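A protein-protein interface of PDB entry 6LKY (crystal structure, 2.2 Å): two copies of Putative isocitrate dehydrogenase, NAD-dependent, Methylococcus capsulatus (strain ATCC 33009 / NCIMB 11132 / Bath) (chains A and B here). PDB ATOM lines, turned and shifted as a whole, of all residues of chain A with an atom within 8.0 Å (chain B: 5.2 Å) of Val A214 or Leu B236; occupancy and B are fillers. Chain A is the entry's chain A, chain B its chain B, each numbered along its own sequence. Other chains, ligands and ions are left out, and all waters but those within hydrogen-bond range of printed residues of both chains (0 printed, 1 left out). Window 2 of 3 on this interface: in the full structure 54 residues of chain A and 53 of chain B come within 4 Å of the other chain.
OD2 of Asp A207 lies close to OD1 of Asp B231 (2.6 Å).
The backbone NH (N) of Ala A208 is in hydrogen-bond range of the side-chain carboxylate (OD2) of Asp B235 (3.5 Å).
O of Asp A207 sits close to OD2 of Asp B235 (3.4 Å).
OG of Ser A210 sits at hydrogen-bond distance from O of Val A206 (2.9 Å).
The side-chain hydroxyl (OG) of Ser B234 lies within hydrogen-bond range of the backbone carbonyl oxygen (O) of Asp B231 (3.1 Å).
Among the printed residues, pairs that only touch across the chains: Val A214 with Gly B239 (3.5 Å), Ser A210 with Ile B232 (3.6 Å), Met A211 with Asp B235 (3.6 Å), Met A215 with Gly B239 (3.6 Å), Ile A232 with Ser B210 (3.6 Å), Leu A236 with Val B214 (3.6 Å), Leu A240 with Val B214 (3.7 Å), Val A214 with Val B214 (3.7 Å), Val A214 with Leu B236 (3.8 Å), Val A214 with Leu B240 (3.9 Å), Met A211 with Gly B239 (3.97 Å) and Val A206 with Ile B232 (3.995 Å).
Of the printed residues of chain B, Ser A210 touches Ile B232 (3.6 Å).
Printed residues of chain B within 4 Å of Met A211: Asp B235 (3.6 Å) and Gly B239 (3.97 Å).
Ala A237 touches none of the printed residues of chain B.
Leu B233 touches none of the printed residues of chain A.
Printed residues of chain A within 4 Å of Leu B236: Val A214 (3.8 Å).
The nearest printed residue of chain B that does not touch Val A214 is Asp B235 (5.2 Å).
Of the 22 printed residues of chain A, 10 touch a printed residue of chain B.
Hydrophobic or aromatic side chains of chain A within 4 Å of the printed part of chain B: Val A206, Met A211, Val A214, Met A215, Ile A232, Leu A236 and Leu A240.
Along chain A the printed residues that touch a printed residue of chain B span positions 206 to 240.
Of the 13 printed residues of chain B, 8 touch a printed residue of chain A.
Among the printed residues, 15 pairs touch across the chains.
Ser A210 touches Ile B232, and with the chains exchanged Ile A232 touches Ser B210.
Val A214 touches its own counterpart, Val B214.
Val A214 touches Leu B236, and with the chains exchanged Leu A236 touches Val B214.
Val A214 touches Leu B240, and with the chains exchanged Leu A240 touches Val B214.
Of the 15 pairs that touch across the chains among the printed residues, 7 have their exchanged pair printed and touching as well.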
ATOM      1  N   ALA A 106     -25.482 -24.411   4.659  1.00  0.00           N
ATOM      2  CA  ALA A 106     -26.343 -24.306   3.484  1.00  0.00           C
ATOM      3  C   ALA A 106     -26.121 -25.466   2.514  1.00  0.00           C
ATOM      4  O   ALA A 106     -27.073 -25.966   1.900  1.00  0.00           O
ATOM      5  CB  ALA A 106     -26.099 -22.974   2.777  1.00  0.00           C
ATOM      6  N   PHE A 107     -24.876 -25.904   2.354  1.00  0.00           N
ATOM      7  CA  PHE A 107     -24.552 -26.943   1.394  1.00  0.00           C
ATOM      8  C   PHE A 107     -24.146 -28.215   2.123  1.00  0.00           C
ATOM      9  O   PHE A 107     -23.625 -28.175   3.243  1.00  0.00           O
ATOM     10  CB  PHE A 107     -23.437 -26.487   0.441  1.00  0.00           C
ATOM     11  CG  PHE A 107     -23.792 -25.251  -0.355  1.00  0.00           C
ATOM     12  CD1 PHE A 107     -24.735 -25.308  -1.372  1.00  0.00           C
ATOM     13  CD2 PHE A 107     -23.199 -24.030  -0.071  1.00  0.00           C
ATOM     14  CE1 PHE A 107     -25.071 -24.172  -2.097  1.00  0.00           C
ATOM     15  CE2 PHE A 107     -23.539 -22.891  -0.788  1.00  0.00           C
ATOM     16  CZ  PHE A 107     -24.470 -22.962  -1.802  1.00  0.00           C
ATOM     17  N   VAL A 206     -10.262 -14.030  -9.450  1.00  0.00           N
ATOM     18  CA  VAL A 206     -10.434 -14.416  -8.045  1.00  0.00           C
ATOM     19  C   VAL A 206     -11.732 -13.865  -7.439  1.00  0.00           C
ATOM     20  O   VAL A 206     -12.365 -14.542  -6.624  1.00  0.00           O
ATOM     21  CB  VAL A 206      -9.186 -14.012  -7.228  1.00  0.00           C
ATOM     22  CG1 VAL A 206      -9.019 -12.480  -7.181  1.00  0.00           C
ATOM     23  CG2 VAL A 206      -9.235 -14.608  -5.828  1.00  0.00           C
ATOM     24  N   ASP A 207     -12.172 -12.655  -7.828  1.00  0.00           N
ATOM     25  CA  ASP A 207     -13.383 -12.100  -7.197  1.00  0.00           C
ATOM     26  C   ASP A 207     -14.656 -12.808  -7.682  1.00  0.00           C
ATOM     27  O   ASP A 207     -15.523 -13.193  -6.873  1.00  0.00           O
ATOM     28  CB  ASP A 207     -13.485 -10.580  -7.424  1.00  0.00           C
ATOM     29  CG  ASP A 207     -13.317 -10.173  -8.893  1.00  0.00           C
ATOM     30  OD1 ASP A 207     -13.053 -11.058  -9.733  1.00  0.00           O
ATOM     31  OD2 ASP A 207     -13.439  -8.958  -9.207  1.00  0.00           O
ATOM     32  N   ALA A 208     -14.783 -13.004  -8.998  1.00  0.00           N
ATOM     33  CA  ALA A 208     -15.885 -13.814  -9.517  1.00  0.00           C
ATOM     34  C   ALA A 208     -15.829 -15.233  -8.959  1.00  0.00           C
ATOM     35  O   ALA A 208     -16.866 -15.836  -8.659  1.00  0.00           O
ATOM     36  CB  ALA A 208     -15.854 -13.830 -11.050  1.00  0.00           C
ATOM     37  N   CYS A 209     -14.620 -15.783  -8.819  1.00  0.00           N
ATOM     38  CA  CYS A 209     -14.477 -17.120  -8.250  1.00  0.00           C
ATOM     39  C   CYS A 209     -14.999 -17.185  -6.816  1.00  0.00           C
ATOM     40  O   CYS A 209     -15.602 -18.187  -6.417  1.00  0.00           O
ATOM     41  CB  CYS A 209     -13.015 -17.546  -8.304  1.00  0.00           C
ATOM     42  SG  CYS A 209     -12.696 -19.230  -7.783  1.00  0.00           S
ATOM     43  N   SER A 210     -14.756 -16.135  -6.023  1.00  0.00           N
ATOM     44  CA  SER A 210     -15.278 -16.112  -4.658  1.00  0.00           C
ATOM     45  C   SER A 210     -16.804 -16.099  -4.657  1.00  0.00           C
ATOM     46  O   SER A 210     -17.446 -16.831  -3.882  1.00  0.00           O
ATOM     47  CB  SER A 210     -14.731 -14.895  -3.908  1.00  0.00           C
ATOM     48  OG  SER A 210     -13.312 -14.868  -3.938  1.00  0.00           O
ATOM     49  N   MET A 211     -17.398 -15.258  -5.516  1.00  0.00           N
ATOM     50  CA  MET A 211     -18.858 -15.247  -5.657  1.00  0.00           C
ATOM     51  C   MET A 211     -19.377 -16.641  -6.015  1.00  0.00           C
ATOM     52  O   MET A 211     -20.323 -17.150  -5.401  1.00  0.00           O
ATOM     53  CB  MET A 211     -19.271 -14.221  -6.718  1.00  0.00           C
ATOM     54  CG  MET A 211     -20.761 -14.236  -7.108  1.00  0.00           C
ATOM     55  SD  MET A 211     -21.154 -15.555  -8.293  1.00  0.00           S
ATOM     56  CE  MET A 211     -20.224 -15.025  -9.757  1.00  0.00           C
ATOM     57  N   GLN A 212     -18.723 -17.291  -6.982  1.00  0.00           N
ATOM     58  CA  GLN A 212     -19.161 -18.607  -7.440  1.00  0.00           C
ATOM     59  C   GLN A 212     -19.020 -19.646  -6.337  1.00  0.00           C
ATOM     60  O   GLN A 212     -19.881 -20.527  -6.190  1.00  0.00           O
ATOM     61  CB  GLN A 212     -18.361 -19.016  -8.683  1.00  0.00           C
ATOM     62  CG  GLN A 212     -18.864 -18.331  -9.978  1.00  0.00           C
ATOM     63  CD  GLN A 212     -17.829 -18.301 -11.121  1.00  0.00           C
ATOM     64  OE1 GLN A 212     -16.884 -19.091 -11.142  1.00  0.00           O
ATOM     65  NE2 GLN A 212     -18.011 -17.370 -12.074  1.00  0.00           N
ATOM     66  N   MET A 213     -17.970 -19.534  -5.521  1.00  0.00           N
ATOM     67  CA  MET A 213     -17.800 -20.478  -4.420  1.00  0.00           C
ATOM     68  C   MET A 213     -18.905 -20.327  -3.385  1.00  0.00           C
ATOM     69  O   MET A 213     -19.388 -21.333  -2.840  1.00  0.00           O
ATOM     70  CB  MET A 213     -16.438 -20.295  -3.763  1.00  0.00           C
ATOM     71  CG  MET A 213     -15.301 -20.801  -4.616  1.00  0.00           C
ATOM     72  SD  MET A 213     -13.711 -20.727  -3.763  1.00  0.00           S
ATOM     73  CE  MET A 213     -14.020 -21.986  -2.504  1.00  0.00           C
ATOM     74  N   VAL A 214     -19.339 -19.097  -3.091  1.00  0.00           N
ATOM     75  CA  VAL A 214     -20.413 -19.022  -2.092  1.00  0.00           C
ATOM     76  C   VAL A 214     -21.771 -19.427  -2.681  1.00  0.00           C
ATOM     77  O   VAL A 214     -22.649 -19.891  -1.942  1.00  0.00           O
ATOM     78  CB  VAL A 214     -20.522 -17.639  -1.417  1.00  0.00           C
ATOM     79  CG1 VAL A 214     -19.262 -17.319  -0.635  1.00  0.00           C
ATOM     80  CG2 VAL A 214     -20.853 -16.548  -2.421  1.00  0.00           C
ATOM     81  N   MET A 215     -21.980 -19.268  -3.992  1.00  0.00           N
ATOM     82  CA  MET A 215     -23.302 -19.562  -4.549  1.00  0.00           C
ATOM     83  C   MET A 215     -23.499 -21.005  -5.024  1.00  0.00           C
ATOM     84  O   MET A 215     -24.614 -21.525  -4.961  1.00  0.00           O
ATOM     85  CB  MET A 215     -23.587 -18.637  -5.724  1.00  0.00           C
ATOM     86  CG  MET A 215     -23.670 -17.201  -5.292  1.00  0.00           C
ATOM     87  SD  MET A 215     -24.197 -16.126  -6.613  1.00  0.00           S
ATOM     88  CE  MET A 215     -25.964 -16.453  -6.598  1.00  0.00           C
ATOM     89  N   GLN A 216     -22.451 -21.648  -5.479  1.00  0.00           N
ATOM     90  CA  GLN A 216     -22.273 -22.921  -6.160  1.00  0.00           C
ATOM     91  C   GLN A 216     -20.917 -23.584  -6.068  1.00  0.00           C
ATOM     92  O   GLN A 216     -20.268 -23.854  -7.085  1.00  0.00           O
ATOM     93  CB  GLN A 216     -22.717 -22.733  -7.583  1.00  0.00           C
ATOM     94  CG  GLN A 216     -23.165 -23.954  -8.295  1.00  0.00           C
ATOM     95  CD  GLN A 216     -23.838 -23.596  -9.547  1.00  0.00           C
ATOM     96  OE1 GLN A 216     -23.198 -23.367 -10.512  1.00  0.00           O
ATOM     97  NE2 GLN A 216     -25.122 -24.170  -9.619  1.00  0.00           N
ATOM     98  N   PRO A 217     -20.550 -23.992  -4.849  1.00  0.00           N
ATOM     99  CA  PRO A 217     -19.252 -24.655  -4.659  1.00  0.00           C
ATOM    100  C   PRO A 217     -19.158 -26.001  -5.360  1.00  0.00           C
ATOM    101  O   PRO A 217     -18.034 -26.480  -5.598  1.00  0.00           O
ATOM    102  CB  PRO A 217     -19.152 -24.807  -3.131  1.00  0.00           C
ATOM    103  CG  PRO A 217     -20.577 -24.660  -2.638  1.00  0.00           C
ATOM    104  CD  PRO A 217     -21.285 -23.803  -3.599  1.00  0.00           C
ATOM    105  N   GLN A 218     -20.294 -26.603  -5.737  1.00  0.00           N
ATOM    106  CA  GLN A 218     -20.270 -27.892  -6.424  1.00  0.00           C
ATOM    107  C   GLN A 218     -19.598 -27.820  -7.784  1.00  0.00           C
ATOM    108  O   GLN A 218     -19.089 -28.840  -8.256  1.00  0.00           O
ATOM    109  CB  GLN A 218     -21.688 -28.448  -6.601  1.00  0.00           C
ATOM    110  CG  GLN A 218     -22.454 -28.619  -5.319  1.00  0.00           C
ATOM    111  CD  GLN A 218     -23.211 -27.358  -4.939  1.00  0.00           C
ATOM    112  OE1 GLN A 218     -23.000 -26.292  -5.527  1.00  0.00           O
ATOM    113  NE2 GLN A 218     -24.099 -27.474  -3.953  1.00  0.00           N
ATOM    114  N   PHE A 220     -16.807 -26.723  -8.369  1.00  0.00           N
ATOM    115  CA  PHE A 220     -15.365 -26.724  -8.201  1.00  0.00           C
ATOM    116  C   PHE A 220     -14.857 -28.114  -7.865  1.00  0.00           C
ATOM    117  O   PHE A 220     -15.496 -28.875  -7.131  1.00  0.00           O
ATOM    118  CB  PHE A 220     -14.942 -25.742  -7.106  1.00  0.00           C
ATOM    119  CG  PHE A 220     -15.113 -24.316  -7.505  1.00  0.00           C
ATOM    120  CD1 PHE A 220     -14.164 -23.682  -8.287  1.00  0.00           C
ATOM    121  CD2 PHE A 220     -16.243 -23.623  -7.136  1.00  0.00           C
ATOM    122  CE1 PHE A 220     -14.335 -22.364  -8.667  1.00  0.00           C
ATOM    123  CE2 PHE A 220     -16.425 -22.309  -7.514  1.00  0.00           C
ATOM    124  CZ  PHE A 220     -15.475 -21.677  -8.279  1.00  0.00           C
ATOM    125  N   ILE A 232      -6.954 -17.258   1.026  1.00  0.00           N
ATOM    126  CA  ILE A 232      -8.286 -16.673   1.164  1.00  0.00           C
ATOM    127  C   ILE A 232      -9.359 -17.668   0.724  1.00  0.00           C
ATOM    128  O   ILE A 232     -10.375 -17.864   1.410  1.00  0.00           O
ATOM    129  CB  ILE A 232      -8.370 -15.361   0.360  1.00  0.00           C
ATOM    130  CG1 ILE A 232      -7.484 -14.280   0.978  1.00  0.00           C
ATOM    131  CG2 ILE A 232      -9.818 -14.871   0.253  1.00  0.00           C
ATOM    132  CD1 ILE A 232      -7.340 -13.041   0.089  1.00  0.00           C
ATOM    133  N   LEU A 233      -9.144 -18.317  -0.421  1.00  0.00           N
ATOM    134  CA  LEU A 233     -10.142 -19.222  -0.980  1.00  0.00           C
ATOM    135  C   LEU A 233     -10.324 -20.458  -0.116  1.00  0.00           C
ATOM    136  O   LEU A 233     -11.455 -20.938   0.059  1.00  0.00           O
ATOM    137  CB  LEU A 233      -9.735 -19.636  -2.391  1.00  0.00           C
ATOM    138  CG  LEU A 233     -10.281 -18.871  -3.594  1.00  0.00           C
ATOM    139  CD1 LEU A 233     -11.039 -17.612  -3.219  1.00  0.00           C
ATOM    140  CD2 LEU A 233      -9.131 -18.556  -4.514  1.00  0.00           C
ATOM    141  N   ASP A 235      -9.908 -20.596   3.100  1.00  0.00           N
ATOM    142  CA  ASP A 235     -10.697 -20.236   4.285  1.00  0.00           C
ATOM    143  C   ASP A 235     -12.174 -20.034   3.943  1.00  0.00           C
ATOM    144  O   ASP A 235     -13.061 -20.358   4.747  1.00  0.00           O
ATOM    145  CB  ASP A 235     -10.134 -18.984   4.943  1.00  0.00           C
ATOM    146  CG  ASP A 235      -8.995 -19.296   5.877  1.00  0.00           C
ATOM    147  OD1 ASP A 235      -8.398 -20.385   5.713  1.00  0.00           O
ATOM    148  OD2 ASP A 235      -8.696 -18.457   6.759  1.00  0.00           O
ATOM    149  N   LEU A 236     -12.454 -19.475   2.767  1.00  0.00           N
ATOM    150  CA  LEU A 236     -13.830 -19.419   2.287  1.00  0.00           C
ATOM    151  C   LEU A 236     -14.443 -20.827   2.250  1.00  0.00           C
ATOM    152  O   LEU A 236     -15.562 -21.053   2.735  1.00  0.00           O
ATOM    153  CB  LEU A 236     -13.842 -18.743   0.906  1.00  0.00           C
ATOM    154  CG  LEU A 236     -15.106 -18.161   0.254  1.00  0.00           C
ATOM    155  CD1 LEU A 236     -14.760 -17.432  -1.050  1.00  0.00           C
ATOM    156  CD2 LEU A 236     -16.154 -19.233  -0.025  1.00  0.00           C
ATOM    157  N   ALA A 237     -13.716 -21.788   1.670  1.00  0.00           N
ATOM    158  CA  ALA A 237     -14.201 -23.169   1.584  1.00  0.00           C
ATOM    159  C   ALA A 237     -14.421 -23.769   2.973  1.00  0.00           C
ATOM    160  O   ALA A 237     -15.428 -24.458   3.220  1.00  0.00           O
ATOM    161  CB  ALA A 237     -13.213 -24.011   0.778  1.00  0.00           C
ATOM    162  N   LEU A 240     -17.588 -22.764   4.115  1.00  0.00           N
ATOM    163  CA  LEU A 240     -18.702 -23.439   3.447  1.00  0.00           C
ATOM    164  C   LEU A 240     -19.011 -24.793   4.071  1.00  0.00           C
ATOM    165  O   LEU A 240     -20.181 -25.190   4.120  1.00  0.00           O
ATOM    166  CB  LEU A 240     -18.426 -23.622   1.955  1.00  0.00           C
ATOM    167  CG  LEU A 240     -18.453 -22.354   1.102  1.00  0.00           C
ATOM    168  CD1 LEU A 240     -17.775 -22.659  -0.238  1.00  0.00           C
ATOM    169  CD2 LEU A 240     -19.866 -21.807   0.910  1.00  0.00           C
ATOM    170  N   SER B 210     -12.989 -13.832   5.550  1.00  0.00           N
ATOM    171  CA  SER B 210     -13.774 -14.473   4.497  1.00  0.00           C
ATOM    172  C   SER B 210     -14.549 -15.664   5.046  1.00  0.00           C
ATOM    173  O   SER B 210     -15.730 -15.863   4.710  1.00  0.00           O
ATOM    174  CB  SER B 210     -12.861 -14.909   3.345  1.00  0.00           C
ATOM    175  OG  SER B 210     -12.125 -13.809   2.827  1.00  0.00           O
ATOM    176  N   MET B 213     -17.489 -14.229   6.881  1.00  0.00           N
ATOM    177  CA  MET B 213     -18.549 -13.734   6.012  1.00  0.00           C
ATOM    178  C   MET B 213     -19.370 -14.880   5.449  1.00  0.00           C
ATOM    179  O   MET B 213     -20.589 -14.760   5.302  1.00  0.00           O
ATOM    180  CB  MET B 213     -17.979 -12.896   4.880  1.00  0.00           C
ATOM    181  CG  MET B 213     -17.518 -11.532   5.353  1.00  0.00           C
ATOM    182  SD  MET B 213     -16.989 -10.456   4.024  1.00  0.00           S
ATOM    183  CE  MET B 213     -18.538 -10.232   3.146  1.00  0.00           C
ATOM    184  N   VAL B 214     -18.720 -15.994   5.110  1.00  0.00           N
ATOM    185  CA  VAL B 214     -19.500 -17.124   4.621  1.00  0.00           C
ATOM    186  C   VAL B 214     -20.383 -17.685   5.737  1.00  0.00           C
ATOM    187  O   VAL B 214     -21.528 -18.089   5.502  1.00  0.00           O
ATOM    188  CB  VAL B 214     -18.572 -18.204   4.032  1.00  0.00           C
ATOM    189  CG1 VAL B 214     -19.366 -19.446   3.692  1.00  0.00           C
ATOM    190  CG2 VAL B 214     -17.865 -17.679   2.797  1.00  0.00           C
ATOM    191  N   ASP B 231     -12.175  -5.687  -3.417  1.00  0.00           N
ATOM    192  CA  ASP B 231     -12.714  -6.350  -4.602  1.00  0.00           C
ATOM    193  C   ASP B 231     -13.237  -7.749  -4.256  1.00  0.00           C
ATOM    194  O   ASP B 231     -14.404  -8.091  -4.536  1.00  0.00           O
ATOM    195  CB  ASP B 231     -11.623  -6.386  -5.681  1.00  0.00           C
ATOM    196  CG  ASP B 231     -12.004  -7.236  -6.882  1.00  0.00           C
ATOM    197  OD1 ASP B 231     -13.159  -7.128  -7.350  1.00  0.00           O
ATOM    198  OD2 ASP B 231     -11.139  -8.008  -7.361  1.00  0.00           O
ATOM    199  N   ILE B 232     -12.413  -8.537  -3.559  1.00  0.00           N
ATOM    200  CA  ILE B 232     -12.777  -9.928  -3.271  1.00  0.00           C
ATOM    201  C   ILE B 232     -13.934  -9.997  -2.280  1.00  0.00           C
ATOM    202  O   ILE B 232     -14.913 -10.730  -2.485  1.00  0.00           O
ATOM    203  CB  ILE B 232     -11.563 -10.710  -2.737  1.00  0.00           C
ATOM    204  CG1 ILE B 232     -10.504 -10.888  -3.831  1.00  0.00           C
ATOM    205  CG2 ILE B 232     -12.020 -12.053  -2.189  1.00  0.00           C
ATOM    206  CD1 ILE B 232      -9.136 -11.355  -3.302  1.00  0.00           C
ATOM    207  N   LEU B 233     -13.839  -9.235  -1.190  1.00  0.00           N
ATOM    208  CA  LEU B 233     -14.851  -9.312  -0.149  1.00  0.00           C
ATOM    209  C   LEU B 233     -16.196  -8.812  -0.655  1.00  0.00           C
ATOM    210  O   LEU B 233     -17.237  -9.381  -0.311  1.00  0.00           O
ATOM    211  CB  LEU B 233     -14.389  -8.531   1.090  1.00  0.00           C
ATOM    212  CG  LEU B 233     -13.566  -9.321   2.123  1.00  0.00           C
ATOM    213  CD1 LEU B 233     -12.333  -9.946   1.519  1.00  0.00           C
ATOM    214  CD2 LEU B 233     -13.152  -8.417   3.274  1.00  0.00           C
ATOM    215  N   SER B 234     -16.208  -7.753  -1.475  1.00  0.00           N
ATOM    216  CA  SER B 234     -17.477  -7.276  -2.000  1.00  0.00           C
ATOM    217  C   SER B 234     -18.087  -8.277  -2.981  1.00  0.00           C
ATOM    218  O   SER B 234     -19.318  -8.416  -3.022  1.00  0.00           O
ATOM    219  CB  SER B 234     -17.304  -5.892  -2.638  1.00  0.00           C
ATOM    220  OG  SER B 234     -16.614  -5.956  -3.877  1.00  0.00           O
ATOM    221  N   ASP B 235     -17.267  -9.029  -3.734  1.00  0.00           N
ATOM    222  CA  ASP B 235     -17.876 -10.054  -4.590  1.00  0.00           C
ATOM    223  C   ASP B 235     -18.416 -11.226  -3.770  1.00  0.00           C
ATOM    224  O   ASP B 235     -19.465 -11.795  -4.105  1.00  0.00           O
ATOM    225  CB  ASP B 235     -16.884 -10.555  -5.635  1.00  0.00           C
ATOM    226  CG  ASP B 235     -16.879  -9.688  -6.894  1.00  0.00           C
ATOM    227  OD1 ASP B 235     -17.141  -8.462  -6.779  1.00  0.00           O
ATOM    228  OD2 ASP B 235     -16.633 -10.236  -7.998  1.00  0.00           O
ATOM    229  N   LEU B 236     -17.717 -11.591  -2.692  1.00  0.00           N
ATOM    230  CA  LEU B 236     -18.226 -12.583  -1.750  1.00  0.00           C
ATOM    231  C   LEU B 236     -19.578 -12.165  -1.183  1.00  0.00           C
ATOM    232  O   LEU B 236     -20.534 -12.957  -1.161  1.00  0.00           O
ATOM    233  CB  LEU B 236     -17.211 -12.780  -0.627  1.00  0.00           C
ATOM    234  CG  LEU B 236     -17.189 -13.995   0.304  1.00  0.00           C
ATOM    235  CD1 LEU B 236     -15.974 -13.879   1.212  1.00  0.00           C
ATOM    236  CD2 LEU B 236     -18.426 -14.100   1.152  1.00  0.00           C
ATOM    237  N   ALA B 237     -19.666 -10.924  -0.693  1.00  0.00           N
ATOM    238  CA  ALA B 237     -20.923 -10.428  -0.145  1.00  0.00           C
ATOM    239  C   ALA B 237     -22.030 -10.440  -1.198  1.00  0.00           C
ATOM    240  O   ALA B 237     -23.188 -10.791  -0.907  1.00  0.00           O
ATOM    241  CB  ALA B 237     -20.726  -9.020   0.411  1.00  0.00           C
ATOM    242  N   ALA B 238     -21.693 -10.044  -2.425  1.00  0.00           N
ATOM    243  CA  ALA B 238     -22.676 -10.107  -3.497  1.00  0.00           C
ATOM    244  C   ALA B 238     -23.197 -11.528  -3.643  1.00  0.00           C
ATOM    245  O   ALA B 238     -24.410 -11.755  -3.734  1.00  0.00           O
ATOM    246  CB  ALA B 238     -22.063  -9.605  -4.805  1.00  0.00           C
ATOM    247  N   GLY B 239     -22.289 -12.500  -3.643  1.00  0.00           N
ATOM    248  CA  GLY B 239     -22.718 -13.881  -3.677  1.00  0.00           C
ATOM    249  C   GLY B 239     -23.671 -14.209  -2.549  1.00  0.00           C
ATOM    250  O   GLY B 239     -24.674 -14.902  -2.749  1.00  0.00           O
ATOM    251  N   LEU B 240     -23.376 -13.706  -1.349  1.00  0.00           N
ATOM    252  CA  LEU B 240     -24.220 -14.012  -0.195  1.00  0.00           C
ATOM    253  C   LEU B 240     -25.637 -13.499  -0.374  1.00  0.00           C
ATOM    254  O   LEU B 240     -26.588 -14.136   0.097  1.00  0.00           O
ATOM    255  CB  LEU B 240     -23.636 -13.411   1.084  1.00  0.00           C
ATOM    256  CG  LEU B 240     -22.422 -14.151   1.627  1.00  0.00           C
ATOM    257  CD1 LEU B 240     -21.711 -13.258   2.638  1.00  0.00           C
ATOM    258  CD2 LEU B 240     -22.831 -15.502   2.242  1.00  0.00           C
